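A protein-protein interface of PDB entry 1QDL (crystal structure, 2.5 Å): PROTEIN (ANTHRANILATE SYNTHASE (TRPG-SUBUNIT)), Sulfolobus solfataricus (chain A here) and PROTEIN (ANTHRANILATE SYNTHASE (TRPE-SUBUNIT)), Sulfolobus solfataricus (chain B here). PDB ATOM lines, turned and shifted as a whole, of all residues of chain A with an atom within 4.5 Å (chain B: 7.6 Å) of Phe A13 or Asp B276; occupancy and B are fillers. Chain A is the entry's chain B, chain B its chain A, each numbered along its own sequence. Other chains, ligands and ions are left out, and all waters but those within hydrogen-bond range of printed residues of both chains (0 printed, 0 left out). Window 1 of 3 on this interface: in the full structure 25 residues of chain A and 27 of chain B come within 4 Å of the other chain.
The side-chain amino group of Lys B340 lies within salt-bridge range of the side-chain carboxylate of Asp B281 (2.8 Å). The backbone NH of Phe B178 lies within hydrogen-bond range of the backbone carbonyl oxygen of Ala B338, 2.6 Å away. The side-chain carboxylate (OD1) of Asp A11 is in hydrogen-bond range of the backbone NH (N) of Val A14 (3.1 Å). ND2 of Asn B280 lies within hydrogen-bond range of OD1 of Asp B281, at 3.2 Å. The side-chain carboxylate of Asp A11 sits at hydrogen-bond distance from the backbone NH of Phe A13. The side-chain carboxylate of Glu A177 lies close to a ring nitrogen (ND1) of His A175, 2.9 Å away.
N of Lys B340 sits at hydrogen-bond distance from OG of Ser A12, at 2.9 Å. The side-chain carboxylate (OD1) of Asp B276 lies close to the backbone NH (N) of Val A179 (3.2 Å). The backbone carbonyl oxygen (O) of Asp B276 lies within hydrogen-bond range of the side-chain amide nitrogen (ND2) of Asn A16, at 3.1 Å. OD2 of Asp B276 is in hydrogen-bond range of OG of Ser A178 (2.6 Å). OD1 of Asn B280 sits at hydrogen-bond distance from N of Tyr A15. The backbone carbonyl oxygen (O) of Arg B279 lies close to the side-chain amide oxygen (OD1) of Asn A16, at 3.3 Å. The backbone NH (N) of Asn B280 sits at hydrogen-bond distance from the side-chain amide oxygen (OD1) of Asn A16 (3.1 Å). NH2 of Arg B279 is in hydrogen-bond range of O of Glu A177 (3.0 Å). OD1 of Asn B280 lies close to O of Ser A12 (3.2 Å). OD1 of Asn B280 lies close to N of Phe A13 (3.3 Å). The side-chain amide oxygen (OD1) of Asn B280 lies within hydrogen-bond range of the backbone NH (N) of Val A14 (3.3 Å). The side-chain carboxylate (OD2) of Asp B276 lies within hydrogen-bond range of the side-chain hydroxyl (OH) of Tyr A135 (2.5 Å).
Phe A13 touches just these residues of chain B: Asp B276 (3.6 Å) and Asn B280 (3.1 Å). Of chain A, only Phe A13, Asn A16, Tyr A135, Ser A178 and Val A179 come within 4 Å of Asp B276. Printed residues of chain B within 4 Å of Glu A177: Arg B279 (3.0 Å). Of the printed residues of chain A, Leu B272 touches Tyr A135 (3.5 Å) and Val A179 (3.9 Å). Asp B281 touches none of the printed residues of chain A. His A175 touches none of the printed residues of chain B. The nearest printed residue of chain A that does not touch Asp B276 is Glu A177 (4.3 Å). The nearest printed residue of chain A that does not touch Leu B272 is Ser A178 (4.3 Å).
Of the 12 printed residues of chain A, 9 touch a printed residue of chain B. Of the 24 printed residues of chain B, 10 touch a printed residue of chain A. Hydrophobic or aromatic side chains of chain B that line the printed part of chain A: Phe B178, Leu B272, Met B273, Val B275 and Val B293. Among the printed residues, 22 pairs touch across the chains.
Ser A12 touches Pro B339. Asp B276 touches Phe A13. CE2 of Phe B178 touches O of Tyr A135 (3.1 Å). Tyr A135 touches Leu B272 (OH to O, 3.5 Å). Met B273 touches Tyr A135 (CA to OH, 3.2 Å). CA of Ser A178 touches NH1 of Arg B279 (3.9 Å). CD1 of Leu B272 touches CG2 of Val A179 (3.9 Å). Val B275 touches Val A179 (CG1 to CG2, 3.8 Å). Arg B279 touches Val A179. CG2 of Val B293 touches CG1 of Val A179, 3.8 Å away.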
ATOM      1  N   ASP A  11      17.873  10.815   3.476  1.00  0.00           N
ATOM      2  CA  ASP A  11      17.406  11.732   2.461  1.00  0.00           C
ATOM      3  C   ASP A  11      16.391  11.212   1.456  1.00  0.00           C
ATOM      4  O   ASP A  11      16.283  10.007   1.222  1.00  0.00           O
ATOM      5  CB  ASP A  11      18.611  12.263   1.705  1.00  0.00           C
ATOM      6  CG  ASP A  11      18.312  13.545   0.992  1.00  0.00           C
ATOM      7  OD1 ASP A  11      18.626  13.634  -0.216  1.00  0.00           O
ATOM      8  OD2 ASP A  11      17.760  14.460   1.644  1.00  0.00           O
ATOM      9  N   SER A  12      15.680  12.161   0.848  1.00  0.00           N
ATOM     10  CA  SER A  12      14.662  11.898  -0.168  1.00  0.00           C
ATOM     11  C   SER A  12      15.137  12.328  -1.575  1.00  0.00           C
ATOM     12  O   SER A  12      14.339  12.429  -2.507  1.00  0.00           O
ATOM     13  CB  SER A  12      13.365  12.642   0.189  1.00  0.00           C
ATOM     14  OG  SER A  12      12.630  11.958   1.197  1.00  0.00           O
ATOM     15  N   PHE A  13      16.435  12.582  -1.722  1.00  0.00           N
ATOM     16  CA  PHE A  13      17.018  12.985  -3.006  1.00  0.00           C
ATOM     17  C   PHE A  13      18.205  12.082  -3.350  1.00  0.00           C
ATOM     18  O   PHE A  13      18.700  12.075  -4.481  1.00  0.00           O
ATOM     19  CB  PHE A  13      17.538  14.421  -2.932  1.00  0.00           C
ATOM     20  CG  PHE A  13      16.476  15.450  -2.726  1.00  0.00           C
ATOM     21  CD1 PHE A  13      16.741  16.587  -1.973  1.00  0.00           C
ATOM     22  CD2 PHE A  13      15.224  15.311  -3.312  1.00  0.00           C
ATOM     23  CE1 PHE A  13      15.769  17.578  -1.810  1.00  0.00           C
ATOM     24  CE2 PHE A  13      14.248  16.294  -3.156  1.00  0.00           C
ATOM     25  CZ  PHE A  13      14.523  17.428  -2.405  1.00  0.00           C
ATOM     26  N   VAL A  14      18.663  11.337  -2.352  1.00  0.00           N
ATOM     27  CA  VAL A  14      19.814  10.464  -2.488  1.00  0.00           C
ATOM     28  C   VAL A  14      19.772   9.516  -3.684  1.00  0.00           C
ATOM     29  O   VAL A  14      20.806   9.270  -4.307  1.00  0.00           O
ATOM     30  CB  VAL A  14      20.049   9.672  -1.168  1.00  0.00           C
ATOM     31  CG1 VAL A  14      18.867   8.769  -0.876  1.00  0.00           C
ATOM     32  CG2 VAL A  14      21.348   8.886  -1.253  1.00  0.00           C
ATOM     33  N   TYR A  15      18.600   8.996  -4.028  1.00  0.00           N
ATOM     34  CA  TYR A  15      18.523   8.086  -5.171  1.00  0.00           C
ATOM     35  C   TYR A  15      18.599   8.793  -6.514  1.00  0.00           C
ATOM     36  O   TYR A  15      18.756   8.155  -7.552  1.00  0.00           O
ATOM     37  CB  TYR A  15      17.270   7.227  -5.086  1.00  0.00           C
ATOM     38  CG  TYR A  15      17.449   6.161  -4.050  1.00  0.00           C
ATOM     39  CD1 TYR A  15      16.982   6.347  -2.752  1.00  0.00           C
ATOM     40  CD2 TYR A  15      18.183   5.013  -4.332  1.00  0.00           C
ATOM     41  CE1 TYR A  15      17.249   5.418  -1.753  1.00  0.00           C
ATOM     42  CE2 TYR A  15      18.455   4.079  -3.343  1.00  0.00           C
ATOM     43  CZ  TYR A  15      17.988   4.284  -2.051  1.00  0.00           C
ATOM     44  OH  TYR A  15      18.274   3.377  -1.050  1.00  0.00           O
ATOM     45  N   ASN A  16      18.483  10.119  -6.492  1.00  0.00           N
ATOM     46  CA  ASN A  16      18.597  10.889  -7.716  1.00  0.00           C
ATOM     47  C   ASN A  16      20.093  10.887  -8.005  1.00  0.00           C
ATOM     48  O   ASN A  16      20.520  10.919  -9.154  1.00  0.00           O
ATOM     49  CB  ASN A  16      18.077  12.317  -7.505  1.00  0.00           C
ATOM     50  CG  ASN A  16      16.563  12.384  -7.516  1.00  0.00           C
ATOM     51  OD1 ASN A  16      15.893  11.494  -8.047  1.00  0.00           O
ATOM     52  ND2 ASN A  16      16.013  13.440  -6.924  1.00  0.00           N
ATOM     53  N   ILE A  17      20.885  10.826  -6.943  1.00  0.00           N
ATOM     54  CA  ILE A  17      22.332  10.780  -7.081  1.00  0.00           C
ATOM     55  C   ILE A  17      22.762   9.385  -7.552  1.00  0.00           C
ATOM     56  O   ILE A  17      23.621   9.247  -8.429  1.00  0.00           O
ATOM     57  CB  ILE A  17      23.038  11.059  -5.742  1.00  0.00           C
ATOM     58  CG1 ILE A  17      22.587  12.407  -5.195  1.00  0.00           C
ATOM     59  CG2 ILE A  17      24.558  11.007  -5.925  1.00  0.00           C
ATOM     60  CD1 ILE A  17      23.096  12.707  -3.799  1.00  0.00           C
ATOM     61  N   TYR A 135      17.797  23.639  -1.652  1.00  0.00           N
ATOM     62  CA  TYR A 135      16.872  23.079  -0.680  1.00  0.00           C
ATOM     63  C   TYR A 135      17.552  23.209   0.673  1.00  0.00           C
ATOM     64  O   TYR A 135      17.949  22.209   1.265  1.00  0.00           O
ATOM     65  CB  TYR A 135      16.638  21.600  -0.967  1.00  0.00           C
ATOM     66  CG  TYR A 135      15.824  21.267  -2.198  1.00  0.00           C
ATOM     67  CD1 TYR A 135      16.443  20.814  -3.372  1.00  0.00           C
ATOM     68  CD2 TYR A 135      14.428  21.312  -2.160  1.00  0.00           C
ATOM     69  CE1 TYR A 135      15.687  20.406  -4.478  1.00  0.00           C
ATOM     70  CE2 TYR A 135      13.663  20.908  -3.255  1.00  0.00           C
ATOM     71  CZ  TYR A 135      14.295  20.455  -4.408  1.00  0.00           C
ATOM     72  OH  TYR A 135      13.526  20.041  -5.471  1.00  0.00           O
ATOM     73  N   HIS A 175      21.849  21.513  -5.644  1.00  0.00           N
ATOM     74  CA  HIS A 175      21.560  20.134  -5.996  1.00  0.00           C
ATOM     75  C   HIS A 175      21.765  19.697  -7.453  1.00  0.00           C
ATOM     76  O   HIS A 175      20.913  19.944  -8.308  1.00  0.00           O
ATOM     77  CB  HIS A 175      20.124  19.827  -5.574  1.00  0.00           C
ATOM     78  CG  HIS A 175      19.934  19.805  -4.093  1.00  0.00           C
ATOM     79  ND1 HIS A 175      19.699  18.641  -3.390  1.00  0.00           N
ATOM     80  CD2 HIS A 175      20.003  20.795  -3.170  1.00  0.00           C
ATOM     81  CE1 HIS A 175      19.639  18.916  -2.097  1.00  0.00           C
ATOM     82  NE2 HIS A 175      19.820  20.215  -1.940  1.00  0.00           N
ATOM     83  N   GLU A 177      21.610  16.757  -8.618  1.00  0.00           N
ATOM     84  CA  GLU A 177      20.654  15.689  -8.943  1.00  0.00           C
ATOM     85  C   GLU A 177      19.258  16.205  -9.227  1.00  0.00           C
ATOM     86  O   GLU A 177      18.367  15.429  -9.575  1.00  0.00           O
ATOM     87  CB  GLU A 177      20.519  14.667  -7.808  1.00  0.00           C
ATOM     88  CG  GLU A 177      21.165  15.051  -6.501  1.00  0.00           C
ATOM     89  CD  GLU A 177      20.427  16.134  -5.737  1.00  0.00           C
ATOM     90  OE1 GLU A 177      19.265  15.934  -5.322  1.00  0.00           O
ATOM     91  OE2 GLU A 177      21.039  17.197  -5.536  1.00  0.00           O
ATOM     92  N   SER A 178      19.056  17.503  -9.061  1.00  0.00           N
ATOM     93  CA  SER A 178      17.740  18.071  -9.282  1.00  0.00           C
ATOM     94  C   SER A 178      17.444  18.362 -10.756  1.00  0.00           C
ATOM     95  O   SER A 178      18.349  18.704 -11.531  1.00  0.00           O
ATOM     96  CB  SER A 178      17.592  19.350  -8.458  1.00  0.00           C
ATOM     97  OG  SER A 178      16.330  19.947  -8.686  1.00  0.00           O
ATOM     98  N   VAL A 179      16.173  18.206 -11.134  1.00  0.00           N
ATOM     99  CA  VAL A 179      15.731  18.493 -12.498  1.00  0.00           C
ATOM    100  C   VAL A 179      15.996  19.970 -12.757  1.00  0.00           C
ATOM    101  O   VAL A 179      16.169  20.386 -13.900  1.00  0.00           O
ATOM    102  CB  VAL A 179      14.210  18.266 -12.696  1.00  0.00           C
ATOM    103  CG1 VAL A 179      13.979  17.180 -13.698  1.00  0.00           C
ATOM    104  CG2 VAL A 179      13.553  17.912 -11.395  1.00  0.00           C
ATOM    105  N   PHE B 178      11.350  20.451   4.874  1.00  0.00           N
ATOM    106  CA  PHE B 178      11.068  21.521   3.941  1.00  0.00           C
ATOM    107  C   PHE B 178       9.572  21.713   4.052  1.00  0.00           C
ATOM    108  O   PHE B 178       9.060  22.829   4.097  1.00  0.00           O
ATOM    109  CB  PHE B 178      11.426  21.097   2.521  1.00  0.00           C
ATOM    110  CG  PHE B 178      12.870  20.783   2.338  1.00  0.00           C
ATOM    111  CD1 PHE B 178      13.266  19.544   1.850  1.00  0.00           C
ATOM    112  CD2 PHE B 178      13.846  21.725   2.664  1.00  0.00           C
ATOM    113  CE1 PHE B 178      14.613  19.240   1.689  1.00  0.00           C
ATOM    114  CE2 PHE B 178      15.201  21.435   2.507  1.00  0.00           C
ATOM    115  CZ  PHE B 178      15.586  20.188   2.019  1.00  0.00           C
ATOM    116  N   PRO B 240       3.291  14.186 -10.034  1.00  0.00           N
ATOM    117  CA  PRO B 240       3.300  15.097  -8.897  1.00  0.00           C
ATOM    118  C   PRO B 240       2.372  16.280  -9.198  1.00  0.00           C
ATOM    119  O   PRO B 240       2.348  16.809 -10.319  1.00  0.00           O
ATOM    120  CB  PRO B 240       4.767  15.516  -8.787  1.00  0.00           C
ATOM    121  CG  PRO B 240       5.522  14.461  -9.523  1.00  0.00           C
ATOM    122  CD  PRO B 240       4.625  14.045 -10.636  1.00  0.00           C
ATOM    123  N   ALA B 269       7.916  26.138  -6.476  1.00  0.00           N
ATOM    124  CA  ALA B 269       8.946  25.607  -5.590  1.00  0.00           C
ATOM    125  C   ALA B 269       8.462  24.318  -4.949  1.00  0.00           C
ATOM    126  O   ALA B 269       9.182  23.322  -4.917  1.00  0.00           O
ATOM    127  CB  ALA B 269       9.292  26.625  -4.520  1.00  0.00           C
ATOM    128  N   GLU B 270       7.237  24.334  -4.442  1.00  0.00           N
ATOM    129  CA  GLU B 270       6.680  23.148  -3.814  1.00  0.00           C
ATOM    130  C   GLU B 270       6.544  22.030  -4.842  1.00  0.00           C
ATOM    131  O   GLU B 270       6.733  20.855  -4.518  1.00  0.00           O
ATOM    132  CB  GLU B 270       5.314  23.472  -3.197  1.00  0.00           C
ATOM    133  CG  GLU B 270       4.266  22.374  -3.374  1.00  0.00           C
ATOM    134  CD  GLU B 270       3.163  22.414  -2.327  1.00  0.00           C
ATOM    135  OE1 GLU B 270       2.647  21.334  -1.961  1.00  0.00           O
ATOM    136  OE2 GLU B 270       2.811  23.526  -1.872  1.00  0.00           O
ATOM    137  N   HIS B 271       6.217  22.395  -6.082  1.00  0.00           N
ATOM    138  CA  HIS B 271       6.052  21.403  -7.141  1.00  0.00           C
ATOM    139  C   HIS B 271       7.385  20.765  -7.515  1.00  0.00           C
ATOM    140  O   HIS B 271       7.485  19.544  -7.682  1.00  0.00           O
ATOM    141  CB  HIS B 271       5.426  22.032  -8.392  1.00  0.00           C
ATOM    142  CG  HIS B 271       4.910  21.024  -9.372  1.00  0.00           C
ATOM    143  ND1 HIS B 271       5.642  20.597 -10.460  1.00  0.00           N
ATOM    144  CD2 HIS B 271       3.748  20.329  -9.409  1.00  0.00           C
ATOM    145  CE1 HIS B 271       4.954  19.684 -11.123  1.00  0.00           C
ATOM    146  NE2 HIS B 271       3.801  19.503 -10.504  1.00  0.00           N
ATOM    147  N   LEU B 272       8.405  21.607  -7.649  1.00  0.00           N
ATOM    148  CA  LEU B 272       9.735  21.143  -8.009  1.00  0.00           C
ATOM    149  C   LEU B 272      10.216  20.104  -7.012  1.00  0.00           C
ATOM    150  O   LEU B 272      10.751  19.060  -7.386  1.00  0.00           O
ATOM    151  CB  LEU B 272      10.714  22.313  -8.038  1.00  0.00           C
ATOM    152  CG  LEU B 272      12.169  21.904  -8.278  1.00  0.00           C
ATOM    153  CD1 LEU B 272      12.250  21.061  -9.534  1.00  0.00           C
ATOM    154  CD2 LEU B 272      13.048  23.133  -8.404  1.00  0.00           C
ATOM    155  N   MET B 273      10.024  20.401  -5.737  1.00  0.00           N
ATOM    156  CA  MET B 273      10.429  19.495  -4.688  1.00  0.00           C
ATOM    157  C   MET B 273       9.708  18.153  -4.822  1.00  0.00           C
ATOM    158  O   MET B 273      10.312  17.090  -4.653  1.00  0.00           O
ATOM    159  CB  MET B 273      10.116  20.122  -3.338  1.00  0.00           C
ATOM    160  CG  MET B 273      10.311  19.200  -2.159  1.00  0.00           C
ATOM    161  SD  MET B 273       9.656  19.915  -0.657  1.00  0.00           S
ATOM    162  CE  MET B 273       7.911  19.334  -0.700  1.00  0.00           C
ATOM    163  N   LEU B 274       8.416  18.204  -5.130  1.00  0.00           N
ATOM    164  CA  LEU B 274       7.613  16.993  -5.274  1.00  0.00           C
ATOM    165  C   LEU B 274       8.085  16.143  -6.447  1.00  0.00           C
ATOM    166  O   LEU B 274       8.072  14.906  -6.386  1.00  0.00           O
ATOM    167  CB  LEU B 274       6.142  17.364  -5.458  1.00  0.00           C
ATOM    168  CG  LEU B 274       5.431  17.694  -4.146  1.00  0.00           C
ATOM    169  CD1 LEU B 274       3.997  18.094  -4.414  1.00  0.00           C
ATOM    170  CD2 LEU B 274       5.477  16.483  -3.235  1.00  0.00           C
ATOM    171  N   VAL B 275       8.492  16.822  -7.517  1.00  0.00           N
ATOM    172  CA  VAL B 275       8.989  16.155  -8.706  1.00  0.00           C
ATOM    173  C   VAL B 275      10.302  15.460  -8.358  1.00  0.00           C
ATOM    174  O   VAL B 275      10.490  14.284  -8.677  1.00  0.00           O
ATOM    175  CB  VAL B 275       9.243  17.163  -9.839  1.00  0.00           C
ATOM    176  CG1 VAL B 275      10.005  16.490 -10.977  1.00  0.00           C
ATOM    177  CG2 VAL B 275       7.920  17.725 -10.329  1.00  0.00           C
ATOM    178  N   ASP B 276      11.205  16.189  -7.701  1.00  0.00           N
ATOM    179  CA  ASP B 276      12.492  15.628  -7.310  1.00  0.00           C
ATOM    180  C   ASP B 276      12.282  14.440  -6.376  1.00  0.00           C
ATOM    181  O   ASP B 276      12.969  13.413  -6.489  1.00  0.00           O
ATOM    182  CB  ASP B 276      13.346  16.695  -6.638  1.00  0.00           C
ATOM    183  CG  ASP B 276      14.151  17.498  -7.645  1.00  0.00           C
ATOM    184  OD1 ASP B 276      14.414  16.969  -8.745  1.00  0.00           O
ATOM    185  OD2 ASP B 276      14.517  18.653  -7.349  1.00  0.00           O
ATOM    186  N   LEU B 277      11.323  14.580  -5.467  1.00  0.00           N
ATOM    187  CA  LEU B 277      10.995  13.520  -4.528  1.00  0.00           C
ATOM    188  C   LEU B 277      10.453  12.324  -5.312  1.00  0.00           C
ATOM    189  O   LEU B 277      10.772  11.178  -5.005  1.00  0.00           O
ATOM    190  CB  LEU B 277       9.947  14.010  -3.523  1.00  0.00           C
ATOM    191  CG  LEU B 277       9.698  13.163  -2.269  1.00  0.00           C
ATOM    192  CD1 LEU B 277       9.443  14.068  -1.079  1.00  0.00           C
ATOM    193  CD2 LEU B 277       8.499  12.245  -2.493  1.00  0.00           C
ATOM    194  N   ALA B 278       9.640  12.598  -6.331  1.00  0.00           N
ATOM    195  CA  ALA B 278       9.064  11.540  -7.165  1.00  0.00           C
ATOM    196  C   ALA B 278      10.135  10.827  -8.010  1.00  0.00           C
ATOM    197  O   ALA B 278      10.114   9.604  -8.166  1.00  0.00           O
ATOM    198  CB  ALA B 278       7.968  12.124  -8.067  1.00  0.00           C
ATOM    199  N   ARG B 279      11.064  11.596  -8.564  1.00  0.00           N
ATOM    200  CA  ARG B 279      12.136  11.020  -9.355  1.00  0.00           C
ATOM    201  C   ARG B 279      13.026  10.181  -8.431  1.00  0.00           C
ATOM    202  O   ARG B 279      13.627   9.191  -8.854  1.00  0.00           O
ATOM    203  CB  ARG B 279      12.964  12.129  -9.997  1.00  0.00           C
ATOM    204  CG  ARG B 279      12.175  13.045 -10.900  1.00  0.00           C
ATOM    205  CD  ARG B 279      12.987  14.273 -11.231  1.00  0.00           C
ATOM    206  NE  ARG B 279      14.341  13.904 -11.621  1.00  0.00           N
ATOM    207  CZ  ARG B 279      15.441  14.270 -10.968  1.00  0.00           C
ATOM    208  NH1 ARG B 279      15.364  15.016  -9.874  1.00  0.00           N
ATOM    209  NH2 ARG B 279      16.624  13.873 -11.403  1.00  0.00           N
ATOM    210  N   ASN B 280      13.107  10.585  -7.168  1.00  0.00           N
ATOM    211  CA  ASN B 280      13.913   9.859  -6.197  1.00  0.00           C
ATOM    212  C   ASN B 280      13.324   8.495  -5.884  1.00  0.00           C
ATOM    213  O   ASN B 280      14.028   7.484  -5.925  1.00  0.00           O
ATOM    214  CB  ASN B 280      14.036  10.641  -4.892  1.00  0.00           C
ATOM    215  CG  ASN B 280      14.789   9.862  -3.819  1.00  0.00           C
ATOM    216  OD1 ASN B 280      16.004   9.988  -3.681  1.00  0.00           O
ATOM    217  ND2 ASN B 280      14.069   9.049  -3.061  1.00  0.00           N
ATOM    218  N   ASP B 281      12.032   8.469  -5.563  1.00  0.00           N
ATOM    219  CA  ASP B 281      11.364   7.215  -5.230  1.00  0.00           C
ATOM    220  C   ASP B 281      11.383   6.247  -6.407  1.00  0.00           C
ATOM    221  O   ASP B 281      11.550   5.036  -6.219  1.00  0.00           O
ATOM    222  CB  ASP B 281       9.923   7.472  -4.770  1.00  0.00           C
ATOM    223  CG  ASP B 281       9.852   8.138  -3.394  1.00  0.00           C
ATOM    224  OD1 ASP B 281      10.912   8.413  -2.793  1.00  0.00           O
ATOM    225  OD2 ASP B 281       8.730   8.394  -2.912  1.00  0.00           O
ATOM    226  N   LEU B 282      11.213   6.768  -7.621  1.00  0.00           N
ATOM    227  CA  LEU B 282      11.252   5.902  -8.794  1.00  0.00           C
ATOM    228  C   LEU B 282      12.699   5.412  -8.896  1.00  0.00           C
ATOM    229  O   LEU B 282      12.956   4.270  -9.278  1.00  0.00           O
ATOM    230  CB  LEU B 282      10.858   6.680 -10.060  1.00  0.00           C
ATOM    231  CG  LEU B 282       9.523   6.319 -10.733  1.00  0.00           C
ATOM    232  CD1 LEU B 282       8.402   6.472  -9.741  1.00  0.00           C
ATOM    233  CD2 LEU B 282       9.255   7.218 -11.928  1.00  0.00           C
ATOM    234  N   GLY B 283      13.628   6.285  -8.505  1.00  0.00           N
ATOM    235  CA  GLY B 283      15.044   5.974  -8.556  1.00  0.00           C
ATOM    236  C   GLY B 283      15.460   4.755  -7.757  1.00  0.00           C
ATOM    237  O   GLY B 283      16.521   4.163  -7.996  1.00  0.00           O
ATOM    238  N   VAL B 291      14.678   7.146 -15.432  1.00  0.00           N
ATOM    239  CA  VAL B 291      13.763   8.031 -14.718  1.00  0.00           C
ATOM    240  C   VAL B 291      13.783   9.401 -15.386  1.00  0.00           C
ATOM    241  O   VAL B 291      14.769  10.131 -15.327  1.00  0.00           O
ATOM    242  CB  VAL B 291      14.136   8.162 -13.220  1.00  0.00           C
ATOM    243  CG1 VAL B 291      13.101   9.027 -12.493  1.00  0.00           C
ATOM    244  CG2 VAL B 291      14.198   6.776 -12.578  1.00  0.00           C
ATOM    245  N   VAL B 293      11.355  13.070 -16.728  1.00  0.00           N
ATOM    246  CA  VAL B 293      10.204  13.941 -16.527  1.00  0.00           C
ATOM    247  C   VAL B 293       9.811  14.479 -17.907  1.00  0.00           C
ATOM    248  O   VAL B 293      10.131  15.621 -18.260  1.00  0.00           O
ATOM    249  CB  VAL B 293      10.535  15.137 -15.595  1.00  0.00           C
ATOM    250  CG1 VAL B 293       9.265  15.935 -15.290  1.00  0.00           C
ATOM    251  CG2 VAL B 293      11.156  14.636 -14.308  1.00  0.00           C
ATOM    252  N   LEU B 296       7.233  18.481 -17.765  1.00  0.00           N
ATOM    253  CA  LEU B 296       7.560  19.172 -16.538  1.00  0.00           C
ATOM    254  C   LEU B 296       6.834  20.489 -16.284  1.00  0.00           C
ATOM    255  O   LEU B 296       6.931  21.427 -17.073  1.00  0.00           O
ATOM    256  CB  LEU B 296       9.067  19.415 -16.495  1.00  0.00           C
ATOM    257  CG  LEU B 296       9.502  20.279 -15.314  1.00  0.00           C
ATOM    258  CD1 LEU B 296       9.360  19.484 -14.032  1.00  0.00           C
ATOM    259  CD2 LEU B 296      10.924  20.739 -15.500  1.00  0.00           C
ATOM    260  N   VAL B 312       6.269  12.031 -14.352  1.00  0.00           N
ATOM    261  CA  VAL B 312       7.549  11.406 -14.046  1.00  0.00           C
ATOM    262  C   VAL B 312       7.443   9.922 -14.340  1.00  0.00           C
ATOM    263  O   VAL B 312       6.523   9.256 -13.870  1.00  0.00           O
ATOM    264  CB  VAL B 312       7.931  11.609 -12.573  1.00  0.00           C
ATOM    265  CG1 VAL B 312       9.255  10.927 -12.276  1.00  0.00           C
ATOM    266  CG2 VAL B 312       8.022  13.094 -12.272  1.00  0.00           C
ATOM    267  N   ALA B 338       8.929  16.320   3.273  1.00  0.00           N
ATOM    268  CA  ALA B 338      10.290  16.130   2.792  1.00  0.00           C
ATOM    269  C   ALA B 338      11.299  16.860   3.656  1.00  0.00           C
ATOM    270  O   ALA B 338      11.080  18.011   4.040  1.00  0.00           O
ATOM    271  CB  ALA B 338      10.400  16.609   1.368  1.00  0.00           C
ATOM    272  N   PRO B 339      12.396  16.186   4.038  1.00  0.00           N
ATOM    273  CA  PRO B 339      12.768  14.793   3.736  1.00  0.00           C
ATOM    274  C   PRO B 339      11.730  13.850   4.341  1.00  0.00           C
ATOM    275  O   PRO B 339      11.395  13.961   5.522  1.00  0.00           O
ATOM    276  CB  PRO B 339      14.132  14.610   4.395  1.00  0.00           C
ATOM    277  CG  PRO B 339      14.569  15.940   4.845  1.00  0.00           C
ATOM    278  CD  PRO B 339      13.443  16.908   4.781  1.00  0.00           C
ATOM    279  N   LYS B 340      11.242  12.909   3.540  1.00  0.00           N
ATOM    280  CA  LYS B 340      10.201  11.999   3.997  1.00  0.00           C
ATOM    281  C   LYS B 340      10.388  11.235   5.317  1.00  0.00           C
ATOM    282  O   LYS B 340       9.451  11.153   6.118  1.00  0.00           O
ATOM    283  CB  LYS B 340       9.848  11.010   2.882  1.00  0.00           C
ATOM    284  CG  LYS B 340       8.398  10.556   2.939  1.00  0.00           C
ATOM    285  CD  LYS B 340       8.091   9.462   1.933  1.00  0.00           C
ATOM    286  CE  LYS B 340       8.123   9.981   0.497  1.00  0.00           C
ATOM    287  NZ  LYS B 340       7.613   8.954  -0.459  1.00  0.00           N
